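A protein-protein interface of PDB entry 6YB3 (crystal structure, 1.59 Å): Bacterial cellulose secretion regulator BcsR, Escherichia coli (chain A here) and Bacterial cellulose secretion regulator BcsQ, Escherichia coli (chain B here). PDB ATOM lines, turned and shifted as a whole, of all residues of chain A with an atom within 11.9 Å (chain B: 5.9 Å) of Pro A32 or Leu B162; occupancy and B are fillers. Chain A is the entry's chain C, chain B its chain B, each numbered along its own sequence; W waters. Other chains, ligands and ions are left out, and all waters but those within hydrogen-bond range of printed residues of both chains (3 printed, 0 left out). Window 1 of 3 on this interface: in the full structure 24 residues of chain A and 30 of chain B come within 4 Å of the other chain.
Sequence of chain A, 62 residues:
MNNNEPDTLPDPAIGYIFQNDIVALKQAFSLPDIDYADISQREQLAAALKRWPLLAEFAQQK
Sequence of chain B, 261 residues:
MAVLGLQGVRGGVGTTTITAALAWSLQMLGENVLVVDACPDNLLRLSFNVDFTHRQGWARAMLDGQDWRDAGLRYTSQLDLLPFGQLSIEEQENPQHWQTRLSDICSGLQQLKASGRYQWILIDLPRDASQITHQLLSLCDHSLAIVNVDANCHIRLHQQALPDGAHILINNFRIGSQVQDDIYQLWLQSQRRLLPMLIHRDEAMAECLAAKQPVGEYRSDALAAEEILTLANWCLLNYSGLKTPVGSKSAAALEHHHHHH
A ring nitrogen (NE2) of His B158 lies within hydrogen-bond range of the side-chain hydroxyl of Tyr A36, at 2.6 Å.
N of Leu B162 sits at hydrogen-bond distance from O of Ser A30, at 2.8 Å.
The backbone carbonyl oxygen of Ala A28 sits at hydrogen-bond distance from the backbone NH of Asp B164.
The side-chain carboxylate (OD1) of Asp B164 lies within hydrogen-bond range of the side-chain hydroxyl (OG) of Ser A30, 2.8 Å away.
The backbone carbonyl oxygen of Val B9 lies within hydrogen-bond range of the side-chain amide nitrogen of Gln B160, 2.9 Å away.
The guanidinium group (NH1) of Arg B127 lies close to the side-chain amide nitrogen (NE2) of Gln B160, at 3.1 Å.
The guanidinium group (NH1) of Arg B156 is in hydrogen-bond range of the side-chain amide oxygen (OE1) of Gln B160, at 2.9 Å.
The backbone NH (N) of Gly A15 sits at hydrogen-bond distance from the backbone carbonyl oxygen (O) of Phe A29 (2.9 Å).
The backbone NH (N) of Phe A29 is in hydrogen-bond range of the backbone carbonyl oxygen (O) of Tyr A16, 2.8 Å away.
The backbone carbonyl oxygen (O) of Gln A27 is in hydrogen-bond range of the backbone NH (N) of Phe A18.
Among the printed residues, merely in contact across the chains: Gln A27 with Pro B163 (3.9 Å), Gln A27 with Asp B164 (3.99 Å), Ala A28 with Pro B163 (3.9 Å), Phe A29 with Ala B161 (3.6 Å), Phe A29 with Leu B162 (3.4 Å), Phe A29 with Pro B163 (3.7 Å), Phe A29 with Asp B164 (3.2 Å), Ser A30 with Ala B161 (3.3 Å), Leu A31 with His B158 (3.99 Å), Leu A31 with Gln B159 (3.5 Å), Leu A31 with Gln B160 (3.6 Å), Pro A32 with Leu B157 (3.2 Å), Pro A32 with Gln B160 (3.4 Å), Pro A32 with Leu B162 (3.8 Å), Asp A33 with Gln B191 (3.9 Å), Ile A34 with Leu B157 (3.5 Å), Ile A34 with His B158 (3.6 Å), Ile A34 with Gln B191 (3.3 Å) and Phe A58 with His B158 (3.4 Å).
Of chain B, only Leu B157 (3.2 Å), Gln B160 (3.4 Å) and Leu B162 (3.8 Å) come within 4 Å of Pro A32.
Leu B162 touches just these residues of chain A: Phe A29, Ser A30 and Pro A32.
No residue of chain A comes within 4 Å of Val B9.
No residue of chain A comes within 4 Å of Ala B145.
Ala B161 touches two residues of chain A.
Pro B163 touches just these residues of chain A: Gln A27, Ala A28 and Phe A29.
Ala B166 touches none of the printed residues of chain A.
Printed residues of chain B within 4 Å of Asp A33: Gln B191 (3.9 Å).
Of the printed residues of chain B, Tyr A36 touches His B158 (2.6 Å).
Of the printed residues of chain B, Leu A31 touches His B158, Gln B159 and Gln B160.
Printed residues of chain B within 4 Å of Ala A28: Pro B163 and Asp B164.
Of the printed residues of chain B, Phe A29 touches Ala B161, Leu B162, Pro B163 and Asp B164.
Arg B193 touches none of the printed residues of chain A.
The nearest residue of chain B that does not touch Pro A32 is Gln B191 (4.5 Å).
The nearest printed residue of chain B that does not touch Ser A30 is Gln B160 (4.6 Å).
Of the 18 printed residues of chain B, 9 touch a printed residue of chain A.
Along chain A the printed residues that touch a printed residue of chain B span positions 27 to 58.
Water W3 lies within hydrogen-bond range of the side-chain amide oxygen (OE1) of Gln B191, the backbone carbonyl oxygen (O) of Asp A33 and the backbone NH (N) of Arg B193.
Water W2 lies within hydrogen-bond range of O of Pro A32 (2.9 Å) and O of Leu B157 (3.0 Å).
Water W1 bridges OH of Tyr A36 (2.9 Å) and NE2 of Gln B191 (3.1 Å).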
ATOM      1  N   GLY A  15     -18.987 -10.583 -25.765  1.00  0.00           N
ATOM      2  CA  GLY A  15     -18.829 -11.883 -25.140  1.00  0.00           C
ATOM      3  C   GLY A  15     -17.402 -12.395 -25.160  1.00  0.00           C
ATOM      4  O   GLY A  15     -17.126 -13.458 -25.720  1.00  0.00           O
ATOM      5  N   TYR A  16     -16.495 -11.632 -24.553  1.00  0.00           N
ATOM      6  CA  TYR A  16     -15.095 -12.024 -24.438  1.00  0.00           C
ATOM      7  C   TYR A  16     -14.416 -11.145 -23.399  1.00  0.00           C
ATOM      8  O   TYR A  16     -14.702  -9.948 -23.311  1.00  0.00           O
ATOM      9  CB  TYR A  16     -14.373 -11.909 -25.788  1.00  0.00           C
ATOM     10  CG  TYR A  16     -12.875 -12.117 -25.717  1.00  0.00           C
ATOM     11  CD1 TYR A  16     -12.336 -13.338 -25.326  1.00  0.00           C
ATOM     12  CD2 TYR A  16     -11.998 -11.094 -26.058  1.00  0.00           C
ATOM     13  CE1 TYR A  16     -10.964 -13.527 -25.264  1.00  0.00           C
ATOM     14  CE2 TYR A  16     -10.629 -11.273 -26.004  1.00  0.00           C
ATOM     15  CZ  TYR A  16     -10.116 -12.490 -25.607  1.00  0.00           C
ATOM     16  OH  TYR A  16      -8.751 -12.664 -25.551  1.00  0.00           O
ATOM     17  N   ILE A  17     -13.523 -11.748 -22.614  1.00  0.00           N
ATOM     18  CA  ILE A  17     -12.725 -11.039 -21.621  1.00  0.00           C
ATOM     19  C   ILE A  17     -11.257 -11.304 -21.929  1.00  0.00           C
ATOM     20  O   ILE A  17     -10.787 -12.444 -21.814  1.00  0.00           O
ATOM     21  CB  ILE A  17     -13.068 -11.463 -20.186  1.00  0.00           C
ATOM     22  CG1 ILE A  17     -14.491 -11.031 -19.824  1.00  0.00           C
ATOM     23  CG2 ILE A  17     -12.068 -10.868 -19.207  1.00  0.00           C
ATOM     24  CD1 ILE A  17     -14.891 -11.380 -18.404  1.00  0.00           C
ATOM     25  N   PHE A  18     -10.536 -10.257 -22.318  1.00  0.00           N
ATOM     26  CA  PHE A  18      -9.097 -10.346 -22.516  1.00  0.00           C
ATOM     27  C   PHE A  18      -8.385 -10.262 -21.173  1.00  0.00           C
ATOM     28  O   PHE A  18      -8.709  -9.414 -20.338  1.00  0.00           O
ATOM     29  CB  PHE A  18      -8.619  -9.222 -23.435  1.00  0.00           C
ATOM     30  CG  PHE A  18      -7.124  -9.123 -23.554  1.00  0.00           C
ATOM     31  CD1 PHE A  18      -6.433  -9.917 -24.454  1.00  0.00           C
ATOM     32  CD2 PHE A  18      -6.411  -8.226 -22.773  1.00  0.00           C
ATOM     33  CE1 PHE A  18      -5.058  -9.824 -24.569  1.00  0.00           C
ATOM     34  CE2 PHE A  18      -5.036  -8.131 -22.881  1.00  0.00           C
ATOM     35  CZ  PHE A  18      -4.359  -8.929 -23.781  1.00  0.00           C
ATOM     36  N   LYS A  26      -8.005  -6.765 -16.809  1.00  0.00           N
ATOM     37  CA  LYS A  26      -8.886  -7.450 -17.741  1.00  0.00           C
ATOM     38  C   LYS A  26      -9.594  -6.430 -18.624  1.00  0.00           C
ATOM     39  O   LYS A  26      -9.844  -5.291 -18.215  1.00  0.00           O
ATOM     40  CB  LYS A  26      -9.911  -8.327 -17.002  1.00  0.00           C
ATOM     41  CG  LYS A  26      -9.292  -9.537 -16.313  1.00  0.00           C
ATOM     42  CD  LYS A  26     -10.332 -10.412 -15.625  1.00  0.00           C
ATOM     43  CE  LYS A  26      -9.665 -11.589 -14.918  1.00  0.00           C
ATOM     44  NZ  LYS A  26     -10.630 -12.443 -14.168  1.00  0.00           N
ATOM     45  N   GLN A  27      -9.897  -6.844 -19.852  1.00  0.00           N
ATOM     46  CA  GLN A  27     -10.613  -6.010 -20.810  1.00  0.00           C
ATOM     47  C   GLN A  27     -11.774  -6.825 -21.362  1.00  0.00           C
ATOM     48  O   GLN A  27     -11.560  -7.797 -22.093  1.00  0.00           O
ATOM     49  CB  GLN A  27      -9.691  -5.531 -21.935  1.00  0.00           C
ATOM     50  CG  GLN A  27     -10.370  -4.611 -22.945  1.00  0.00           C
ATOM     51  CD  GLN A  27     -10.932  -3.352 -22.303  1.00  0.00           C
ATOM     52  OE1 GLN A  27     -10.196  -2.549 -21.736  1.00  0.00           O
ATOM     53  NE2 GLN A  27     -12.242  -3.179 -22.390  1.00  0.00           N
ATOM     54  N   ALA A  28     -12.992  -6.440 -20.997  1.00  0.00           N
ATOM     55  CA  ALA A  28     -14.194  -7.084 -21.500  1.00  0.00           C
ATOM     56  C   ALA A  28     -14.659  -6.410 -22.785  1.00  0.00           C
ATOM     57  O   ALA A  28     -14.535  -5.191 -22.947  1.00  0.00           O
ATOM     58  CB  ALA A  28     -15.307  -7.032 -20.450  1.00  0.00           C
ATOM     59  N   PHE A  29     -15.192  -7.217 -23.696  1.00  0.00           N
ATOM     60  CA  PHE A  29     -15.767  -6.748 -24.948  1.00  0.00           C
ATOM     61  C   PHE A  29     -17.193  -7.267 -25.065  1.00  0.00           C
ATOM     62  O   PHE A  29     -17.490  -8.385 -24.630  1.00  0.00           O
ATOM     63  CB  PHE A  29     -14.940  -7.230 -26.142  1.00  0.00           C
ATOM     64  CG  PHE A  29     -13.552  -6.658 -26.197  1.00  0.00           C
ATOM     65  CD1 PHE A  29     -12.485  -7.325 -25.609  1.00  0.00           C
ATOM     66  CD2 PHE A  29     -13.309  -5.463 -26.850  1.00  0.00           C
ATOM     67  CE1 PHE A  29     -11.202  -6.798 -25.667  1.00  0.00           C
ATOM     68  CE2 PHE A  29     -12.034  -4.933 -26.915  1.00  0.00           C
ATOM     69  CZ  PHE A  29     -10.978  -5.597 -26.324  1.00  0.00           C
ATOM     70  N   SER A  30     -18.076  -6.464 -25.658  1.00  0.00           N
ATOM     71  CA  SER A  30     -19.438  -6.915 -25.902  1.00  0.00           C
ATOM     72  C   SER A  30     -20.021  -6.156 -27.082  1.00  0.00           C
ATOM     73  O   SER A  30     -19.529  -5.089 -27.464  1.00  0.00           O
ATOM     74  CB  SER A  30     -20.325  -6.745 -24.664  1.00  0.00           C
ATOM     75  OG  SER A  30     -20.287  -5.411 -24.188  1.00  0.00           O
ATOM     76  N   LEU A  31     -21.080  -6.723 -27.657  1.00  0.00           N
ATOM     77  CA  LEU A  31     -21.771  -6.057 -28.751  1.00  0.00           C
ATOM     78  C   LEU A  31     -22.357  -4.731 -28.269  1.00  0.00           C
ATOM     79  O   LEU A  31     -22.788  -4.620 -27.117  1.00  0.00           O
ATOM     80  CB  LEU A  31     -22.890  -6.937 -29.310  1.00  0.00           C
ATOM     81  CG  LEU A  31     -22.499  -8.192 -30.089  1.00  0.00           C
ATOM     82  CD1 LEU A  31     -23.738  -8.860 -30.665  1.00  0.00           C
ATOM     83  CD2 LEU A  31     -21.514  -7.853 -31.191  1.00  0.00           C
ATOM     84  N   PRO A  32     -22.377  -3.711 -29.128  1.00  0.00           N
ATOM     85  CA  PRO A  32     -22.980  -2.428 -28.744  1.00  0.00           C
ATOM     86  C   PRO A  32     -24.436  -2.580 -28.323  1.00  0.00           C
ATOM     87  O   PRO A  32     -25.153  -3.474 -28.780  1.00  0.00           O
ATOM     88  CB  PRO A  32     -22.859  -1.587 -30.021  1.00  0.00           C
ATOM     89  CG  PRO A  32     -21.693  -2.180 -30.744  1.00  0.00           C
ATOM     90  CD  PRO A  32     -21.770  -3.659 -30.469  1.00  0.00           C
ATOM     91  N   ASP A  33     -24.867  -1.681 -27.438  1.00  0.00           N
ATOM     92  CA  ASP A  33     -26.209  -1.731 -26.867  1.00  0.00           C
ATOM     93  C   ASP A  33     -27.196  -1.111 -27.849  1.00  0.00           C
ATOM     94  O   ASP A  33     -27.215   0.111 -28.029  1.00  0.00           O
ATOM     95  CB  ASP A  33     -26.226  -0.997 -25.530  1.00  0.00           C
ATOM     96  CG  ASP A  33     -27.497  -1.233 -24.754  1.00  0.00           C
ATOM     97  OD1 ASP A  33     -28.240  -2.174 -25.105  1.00  0.00           O
ATOM     98  OD2 ASP A  33     -27.757  -0.471 -23.796  1.00  0.00           O
ATOM     99  N   ILE A  34     -28.022  -1.942 -28.481  1.00  0.00           N
ATOM    100  CA  ILE A  34     -28.970  -1.485 -29.493  1.00  0.00           C
ATOM    101  C   ILE A  34     -30.377  -1.899 -29.085  1.00  0.00           C
ATOM    102  O   ILE A  34     -30.611  -3.062 -28.731  1.00  0.00           O
ATOM    103  CB  ILE A  34     -28.630  -2.037 -30.886  1.00  0.00           C
ATOM    104  CG1 ILE A  34     -27.191  -1.699 -31.268  1.00  0.00           C
ATOM    105  CG2 ILE A  34     -29.603  -1.470 -31.911  1.00  0.00           C
ATOM    106  CD1 ILE A  34     -26.767  -2.270 -32.622  1.00  0.00           C
ATOM    107  N   ASP A  35     -31.314  -0.952 -29.165  1.00  0.00           N
ATOM    108  CA  ASP A  35     -32.698  -1.158 -28.747  1.00  0.00           C
ATOM    109  C   ASP A  35     -33.628  -0.767 -29.889  1.00  0.00           C
ATOM    110  O   ASP A  35     -33.754   0.419 -30.210  1.00  0.00           O
ATOM    111  CB  ASP A  35     -33.010  -0.340 -27.495  1.00  0.00           C
ATOM    112  CG  ASP A  35     -34.434  -0.520 -27.024  1.00  0.00           C
ATOM    113  OD1 ASP A  35     -35.083  -1.505 -27.443  1.00  0.00           O
ATOM    114  OD2 ASP A  35     -34.904   0.326 -26.237  1.00  0.00           O
ATOM    115  N   TYR A  36     -34.295  -1.756 -30.486  1.00  0.00           N
ATOM    116  CA  TYR A  36     -35.250  -1.522 -31.562  1.00  0.00           C
ATOM    117  C   TYR A  36     -36.703  -1.558 -31.092  1.00  0.00           C
ATOM    118  O   TYR A  36     -37.611  -1.616 -31.928  1.00  0.00           O
ATOM    119  CB  TYR A  36     -35.047  -2.548 -32.685  1.00  0.00           C
ATOM    120  CG  TYR A  36     -33.804  -2.328 -33.521  1.00  0.00           C
ATOM    121  CD1 TYR A  36     -33.658  -1.180 -34.285  1.00  0.00           C
ATOM    122  CD2 TYR A  36     -32.783  -3.275 -33.559  1.00  0.00           C
ATOM    123  CE1 TYR A  36     -32.532  -0.972 -35.055  1.00  0.00           C
ATOM    124  CE2 TYR A  36     -31.648  -3.075 -34.332  1.00  0.00           C
ATOM    125  CZ  TYR A  36     -31.528  -1.922 -35.075  1.00  0.00           C
ATOM    126  OH  TYR A  36     -30.409  -1.699 -35.845  1.00  0.00           O
ATOM    127  N   PHE A  58     -32.031  -5.811 -39.600  1.00  0.00           N
ATOM    128  CA  PHE A  58     -31.581  -5.758 -38.211  1.00  0.00           C
ATOM    129  C   PHE A  58     -32.706  -5.367 -37.262  1.00  0.00           C
ATOM    130  O   PHE A  58     -32.742  -5.846 -36.120  1.00  0.00           O
ATOM    131  CB  PHE A  58     -30.414  -4.784 -38.066  1.00  0.00           C
ATOM    132  CG  PHE A  58     -29.164  -5.213 -38.784  1.00  0.00           C
ATOM    133  CD1 PHE A  58     -28.390  -6.252 -38.293  1.00  0.00           C
ATOM    134  CD2 PHE A  58     -28.753  -4.561 -39.934  1.00  0.00           C
ATOM    135  CE1 PHE A  58     -27.234  -6.639 -38.941  1.00  0.00           C
ATOM    136  CE2 PHE A  58     -27.592  -4.941 -40.587  1.00  0.00           C
ATOM    137  CZ  PHE A  58     -26.835  -5.986 -40.089  1.00  0.00           C
ATOM    138  N   GLN A  61     -35.237  -8.306 -36.332  1.00  0.00           N
ATOM    139  CA  GLN A  61     -34.664  -9.162 -35.302  1.00  0.00           C
ATOM    140  C   GLN A  61     -34.709  -8.460 -33.949  1.00  0.00           C
ATOM    141  O   GLN A  61     -34.402  -9.058 -32.920  1.00  0.00           O
ATOM    142  CB  GLN A  61     -33.223  -9.538 -35.654  1.00  0.00           C
ATOM    143  CG  GLN A  61     -33.067 -10.236 -36.997  1.00  0.00           C
ATOM    144  CD  GLN A  61     -31.628 -10.244 -37.487  1.00  0.00           C
ATOM    145  OE1 GLN A  61     -31.369 -10.112 -38.684  1.00  0.00           O
ATOM    146  NE2 GLN A  61     -30.686 -10.398 -36.561  1.00  0.00           N
ATOM    147  N   GLN B   7     -10.688   4.436 -30.839  1.00  0.00           N
ATOM    148  CA  GLN B   7     -10.522   3.311 -31.752  1.00  0.00           C
ATOM    149  C   GLN B   7     -11.615   3.358 -32.808  1.00  0.00           C
ATOM    150  O   GLN B   7     -12.800   3.445 -32.477  1.00  0.00           O
ATOM    151  CB  GLN B   7     -10.573   1.984 -30.996  1.00  0.00           C
ATOM    152  CG  GLN B   7     -10.189   0.813 -31.887  1.00  0.00           C
ATOM    153  CD  GLN B   7     -10.292  -0.504 -31.164  1.00  0.00           C
ATOM    154  OE1 GLN B   7     -11.236  -0.736 -30.406  1.00  0.00           O
ATOM    155  NE2 GLN B   7      -9.300  -1.369 -31.367  1.00  0.00           N
ATOM    156  N   VAL B   9     -14.251   1.957 -35.395  1.00  0.00           N
ATOM    157  CA  VAL B   9     -15.032   0.739 -35.604  1.00  0.00           C
ATOM    158  C   VAL B   9     -14.601   0.084 -36.909  1.00  0.00           C
ATOM    159  O   VAL B   9     -14.686  -1.140 -37.064  1.00  0.00           O
ATOM    160  CB  VAL B   9     -16.537   1.074 -35.559  1.00  0.00           C
ATOM    161  CG1 VAL B   9     -17.395  -0.055 -36.081  1.00  0.00           C
ATOM    162  CG2 VAL B   9     -16.942   1.420 -34.114  1.00  0.00           C
ATOM    163  N   ARG B 127      -7.401  -0.438 -35.584  1.00  0.00           N
ATOM    164  CA  ARG B 127      -8.496  -1.371 -35.840  1.00  0.00           C
ATOM    165  C   ARG B 127      -7.899  -2.754 -36.109  1.00  0.00           C
ATOM    166  O   ARG B 127      -7.851  -3.249 -37.234  1.00  0.00           O
ATOM    167  CB  ARG B 127      -9.344  -0.868 -37.006  1.00  0.00           C
ATOM    168  CG  ARG B 127     -10.481  -1.792 -37.482  1.00  0.00           C
ATOM    169  CD  ARG B 127     -11.614  -1.858 -36.481  1.00  0.00           C
ATOM    170  NE  ARG B 127     -11.452  -2.949 -35.525  1.00  0.00           N
ATOM    171  CZ  ARG B 127     -12.024  -2.976 -34.324  1.00  0.00           C
ATOM    172  NH1 ARG B 127     -12.780  -1.967 -33.924  1.00  0.00           N
ATOM    173  NH2 ARG B 127     -11.831  -4.007 -33.517  1.00  0.00           N
ATOM    174  N   ALA B 145     -15.484   4.978 -29.602  1.00  0.00           N
ATOM    175  CA  ALA B 145     -15.520   4.150 -30.800  1.00  0.00           C
ATOM    176  C   ALA B 145     -15.969   5.046 -31.948  1.00  0.00           C
ATOM    177  O   ALA B 145     -17.100   5.539 -31.950  1.00  0.00           O
ATOM    178  CB  ALA B 145     -16.462   2.964 -30.604  1.00  0.00           C
ATOM    179  N   ARG B 156     -21.473  -3.244 -38.782  1.00  0.00           N
ATOM    180  CA  ARG B 156     -20.423  -3.594 -37.831  1.00  0.00           C
ATOM    181  C   ARG B 156     -20.929  -3.481 -36.404  1.00  0.00           C
ATOM    182  O   ARG B 156     -20.576  -4.299 -35.550  1.00  0.00           O
ATOM    183  CB  ARG B 156     -19.193  -2.706 -38.046  1.00  0.00           C
ATOM    184  CG  ARG B 156     -18.356  -3.079 -39.281  1.00  0.00           C
ATOM    185  CD  ARG B 156     -17.188  -2.109 -39.457  1.00  0.00           C
ATOM    186  NE  ARG B 156     -16.291  -2.510 -40.536  1.00  0.00           N
ATOM    187  CZ  ARG B 156     -15.251  -3.325 -40.369  1.00  0.00           C
ATOM    188  NH1 ARG B 156     -14.975  -3.814 -39.164  1.00  0.00           N
ATOM    189  NH2 ARG B 156     -14.478  -3.653 -41.403  1.00  0.00           N
ATOM    190  N   LEU B 157     -21.802  -2.506 -36.141  1.00  0.00           N
ATOM    191  CA  LEU B 157     -22.331  -2.314 -34.796  1.00  0.00           C
ATOM    192  C   LEU B 157     -23.263  -3.440 -34.355  1.00  0.00           C
ATOM    193  O   LEU B 157     -23.579  -3.521 -33.162  1.00  0.00           O
ATOM    194  CB  LEU B 157     -23.047  -0.965 -34.708  1.00  0.00           C
ATOM    195  CG  LEU B 157     -22.170   0.293 -34.763  1.00  0.00           C
ATOM    196  CD1 LEU B 157     -23.048   1.555 -34.757  1.00  0.00           C
ATOM    197  CD2 LEU B 157     -21.188   0.340 -33.597  1.00  0.00           C
ATOM    198  N   HIS B 158     -23.700  -4.314 -35.265  1.00  0.00           N
ATOM    199  CA  HIS B 158     -24.507  -5.473 -34.896  1.00  0.00           C
ATOM    200  C   HIS B 158     -23.702  -6.759 -34.800  1.00  0.00           C
ATOM    201  O   HIS B 158     -24.275  -7.806 -34.477  1.00  0.00           O
ATOM    202  CB  HIS B 158     -25.648  -5.676 -35.899  1.00  0.00           C
ATOM    203  CG  HIS B 158     -26.583  -4.512 -35.987  1.00  0.00           C
ATOM    204  ND1 HIS B 158     -26.289  -3.378 -36.713  1.00  0.00           N
ATOM    205  CD2 HIS B 158     -27.808  -4.306 -35.446  1.00  0.00           C
ATOM    206  CE1 HIS B 158     -27.294  -2.523 -36.617  1.00  0.00           C
ATOM    207  NE2 HIS B 158     -28.232  -3.066 -35.860  1.00  0.00           N
ATOM    208  N   GLN B 159     -22.396  -6.720 -35.071  1.00  0.00           N
ATOM    209  CA  GLN B 159     -21.638  -7.969 -35.117  1.00  0.00           C
ATOM    210  C   GLN B 159     -20.250  -7.912 -34.501  1.00  0.00           C
ATOM    211  O   GLN B 159     -19.684  -8.979 -34.253  1.00  0.00           O
ATOM    212  CB  GLN B 159     -21.500  -8.461 -36.562  1.00  0.00           C
ATOM    213  CG  GLN B 159     -20.601  -7.605 -37.429  1.00  0.00           C
ATOM    214  CD  GLN B 159     -20.411  -8.187 -38.819  1.00  0.00           C
ATOM    215  OE1 GLN B 159     -21.206  -9.015 -39.274  1.00  0.00           O
ATOM    216  NE2 GLN B 159     -19.353  -7.759 -39.498  1.00  0.00           N
ATOM    217  N   GLN B 160     -19.655  -6.749 -34.245  1.00  0.00           N
ATOM    218  CA  GLN B 160     -18.332  -6.735 -33.643  1.00  0.00           C
ATOM    219  C   GLN B 160     -18.415  -6.108 -32.260  1.00  0.00           C
ATOM    220  O   GLN B 160     -19.195  -5.180 -32.030  1.00  0.00           O
ATOM    221  CB  GLN B 160     -17.291  -6.023 -34.535  1.00  0.00           C
ATOM    222  CG  GLN B 160     -17.257  -4.531 -34.473  1.00  0.00           C
ATOM    223  CD  GLN B 160     -16.299  -3.931 -35.496  1.00  0.00           C
ATOM    224  OE1 GLN B 160     -16.339  -4.276 -36.675  1.00  0.00           O
ATOM    225  NE2 GLN B 160     -15.447  -3.011 -35.047  1.00  0.00           N
ATOM    226  N   ALA B 161     -17.658  -6.680 -31.334  1.00  0.00           N
ATOM    227  CA  ALA B 161     -17.651  -6.213 -29.960  1.00  0.00           C
ATOM    228  C   ALA B 161     -16.890  -4.902 -29.851  1.00  0.00           C
ATOM    229  O   ALA B 161     -15.900  -4.675 -30.554  1.00  0.00           O
ATOM    230  CB  ALA B 161     -17.018  -7.260 -29.044  1.00  0.00           C
ATOM    231  N   LEU B 162     -17.362  -4.043 -28.972  1.00  0.00           N
ATOM    232  CA  LEU B 162     -16.641  -2.845 -28.615  1.00  0.00           C
ATOM    233  C   LEU B 162     -16.143  -2.972 -27.186  1.00  0.00           C
ATOM    234  O   LEU B 162     -16.656  -3.789 -26.413  1.00  0.00           O
ATOM    235  CB  LEU B 162     -17.536  -1.606 -28.741  1.00  0.00           C
ATOM    236  CG  LEU B 162     -18.060  -1.313 -30.145  1.00  0.00           C
ATOM    237  CD1 LEU B 162     -18.704   0.055 -30.156  1.00  0.00           C
ATOM    238  CD2 LEU B 162     -16.943  -1.410 -31.176  1.00  0.00           C
ATOM    239  N   PRO B 163     -15.124  -2.206 -26.807  1.00  0.00           N
ATOM    240  CA  PRO B 163     -14.711  -2.188 -25.402  1.00  0.00           C
ATOM    241  C   PRO B 163     -15.910  -1.861 -24.526  1.00  0.00           C
ATOM    242  O   PRO B 163     -16.724  -1.001 -24.864  1.00  0.00           O
ATOM    243  CB  PRO B 163     -13.653  -1.082 -25.360  1.00  0.00           C
ATOM    244  CG  PRO B 163     -13.126  -1.014 -26.743  1.00  0.00           C
ATOM    245  CD  PRO B 163     -14.282  -1.331 -27.643  1.00  0.00           C
ATOM    246  N   ASP B 164     -16.053  -2.595 -23.422  1.00  0.00           N
ATOM    247  CA  ASP B 164     -17.192  -2.369 -22.540  1.00  0.00           C
ATOM    248  C   ASP B 164     -17.221  -0.920 -22.070  1.00  0.00           C
ATOM    249  O   ASP B 164     -16.193  -0.354 -21.686  1.00  0.00           O
ATOM    250  CB  ASP B 164     -17.145  -3.320 -21.343  1.00  0.00           C
ATOM    251  CG  ASP B 164     -17.759  -4.676 -21.653  1.00  0.00           C
ATOM    252  OD1 ASP B 164     -17.906  -5.005 -22.851  1.00  0.00           O
ATOM    253  OD2 ASP B 164     -18.105  -5.407 -20.701  1.00  0.00           O
ATOM    254  N   GLY B 165     -18.407  -0.313 -22.126  1.00  0.00           N
ATOM    255  CA  GLY B 165     -18.589   1.066 -21.729  1.00  0.00           C
ATOM    256  C   GLY B 165     -18.232   2.101 -22.774  1.00  0.00           C
ATOM    257  O   GLY B 165     -18.432   3.297 -22.526  1.00  0.00           O
ATOM    258  N   ALA B 166     -17.707   1.693 -23.927  1.00  0.00           N
ATOM    259  CA  ALA B 166     -17.346   2.658 -24.953  1.00  0.00           C
ATOM    260  C   ALA B 166     -18.566   3.460 -25.386  1.00  0.00           C
ATOM    261  O   ALA B 166     -19.695   2.965 -25.387  1.00  0.00           O
ATOM    262  CB  ALA B 166     -16.738   1.948 -26.165  1.00  0.00           C
ATOM    263  N   ILE B 168     -19.995   5.944 -28.676  1.00  0.00           N
ATOM    264  CA  ILE B 168     -19.855   5.995 -30.124  1.00  0.00           C
ATOM    265  C   ILE B 168     -19.861   7.453 -30.562  1.00  0.00           C
ATOM    266  O   ILE B 168     -20.775   8.208 -30.213  1.00  0.00           O
ATOM    267  CB  ILE B 168     -20.989   5.210 -30.808  1.00  0.00           C
ATOM    268  CG1 ILE B 168     -20.977   3.755 -30.331  1.00  0.00           C
ATOM    269  CG2 ILE B 168     -20.871   5.323 -32.316  1.00  0.00           C
ATOM    270  CD1 ILE B 168     -22.223   2.924 -30.697  1.00  0.00           C
ATOM    271  N   GLN B 191     -29.493   3.419 -30.844  1.00  0.00           N
ATOM    272  CA  GLN B 191     -28.104   3.196 -30.445  1.00  0.00           C
ATOM    273  C   GLN B 191     -27.873   3.819 -29.073  1.00  0.00           C
ATOM    274  O   GLN B 191     -27.596   5.016 -28.964  1.00  0.00           O
ATOM    275  CB  GLN B 191     -27.150   3.778 -31.479  1.00  0.00           C
ATOM    276  CG  GLN B 191     -27.160   3.045 -32.814  1.00  0.00           C
ATOM    277  CD  GLN B 191     -26.387   1.736 -32.765  1.00  0.00           C
ATOM    278  OE1 GLN B 191     -25.566   1.514 -31.867  1.00  0.00           O
ATOM    279  NE2 GLN B 191     -26.646   0.861 -33.733  1.00  0.00           N
ATOM    280  N   ARG B 193     -25.515   3.851 -26.998  1.00  0.00           N
ATOM    281  CA  ARG B 193     -24.198   4.369 -26.652  1.00  0.00           C
ATOM    282  C   ARG B 193     -23.782   5.569 -27.502  1.00  0.00           C
ATOM    283  O   ARG B 193     -22.629   6.009 -27.415  1.00  0.00           O
ATOM    284  CB  ARG B 193     -23.152   3.256 -26.771  1.00  0.00           C
ATOM    285  CG  ARG B 193     -23.517   1.961 -26.028  1.00  0.00           C
ATOM    286  CD  ARG B 193     -23.687   2.194 -24.525  1.00  0.00           C
ATOM    287  NE  ARG B 193     -22.449   2.655 -23.903  1.00  0.00           N
ATOM    288  CZ  ARG B 193     -22.304   2.889 -22.602  1.00  0.00           C
ATOM    289  NH1 ARG B 193     -23.326   2.707 -21.774  1.00  0.00           N
ATOM    290  NH2 ARG B 193     -21.138   3.310 -22.128  1.00  0.00           N
HETATM  291  O   HOH W   1     -29.414   0.937 -35.139  1.00  0.00           O
HETATM  292  O   HOH W   2     -25.120  -5.135 -31.106  1.00  0.00           O
HETATM  293  O   HOH W   3     -25.198   1.763 -29.129  1.00  0.00           O
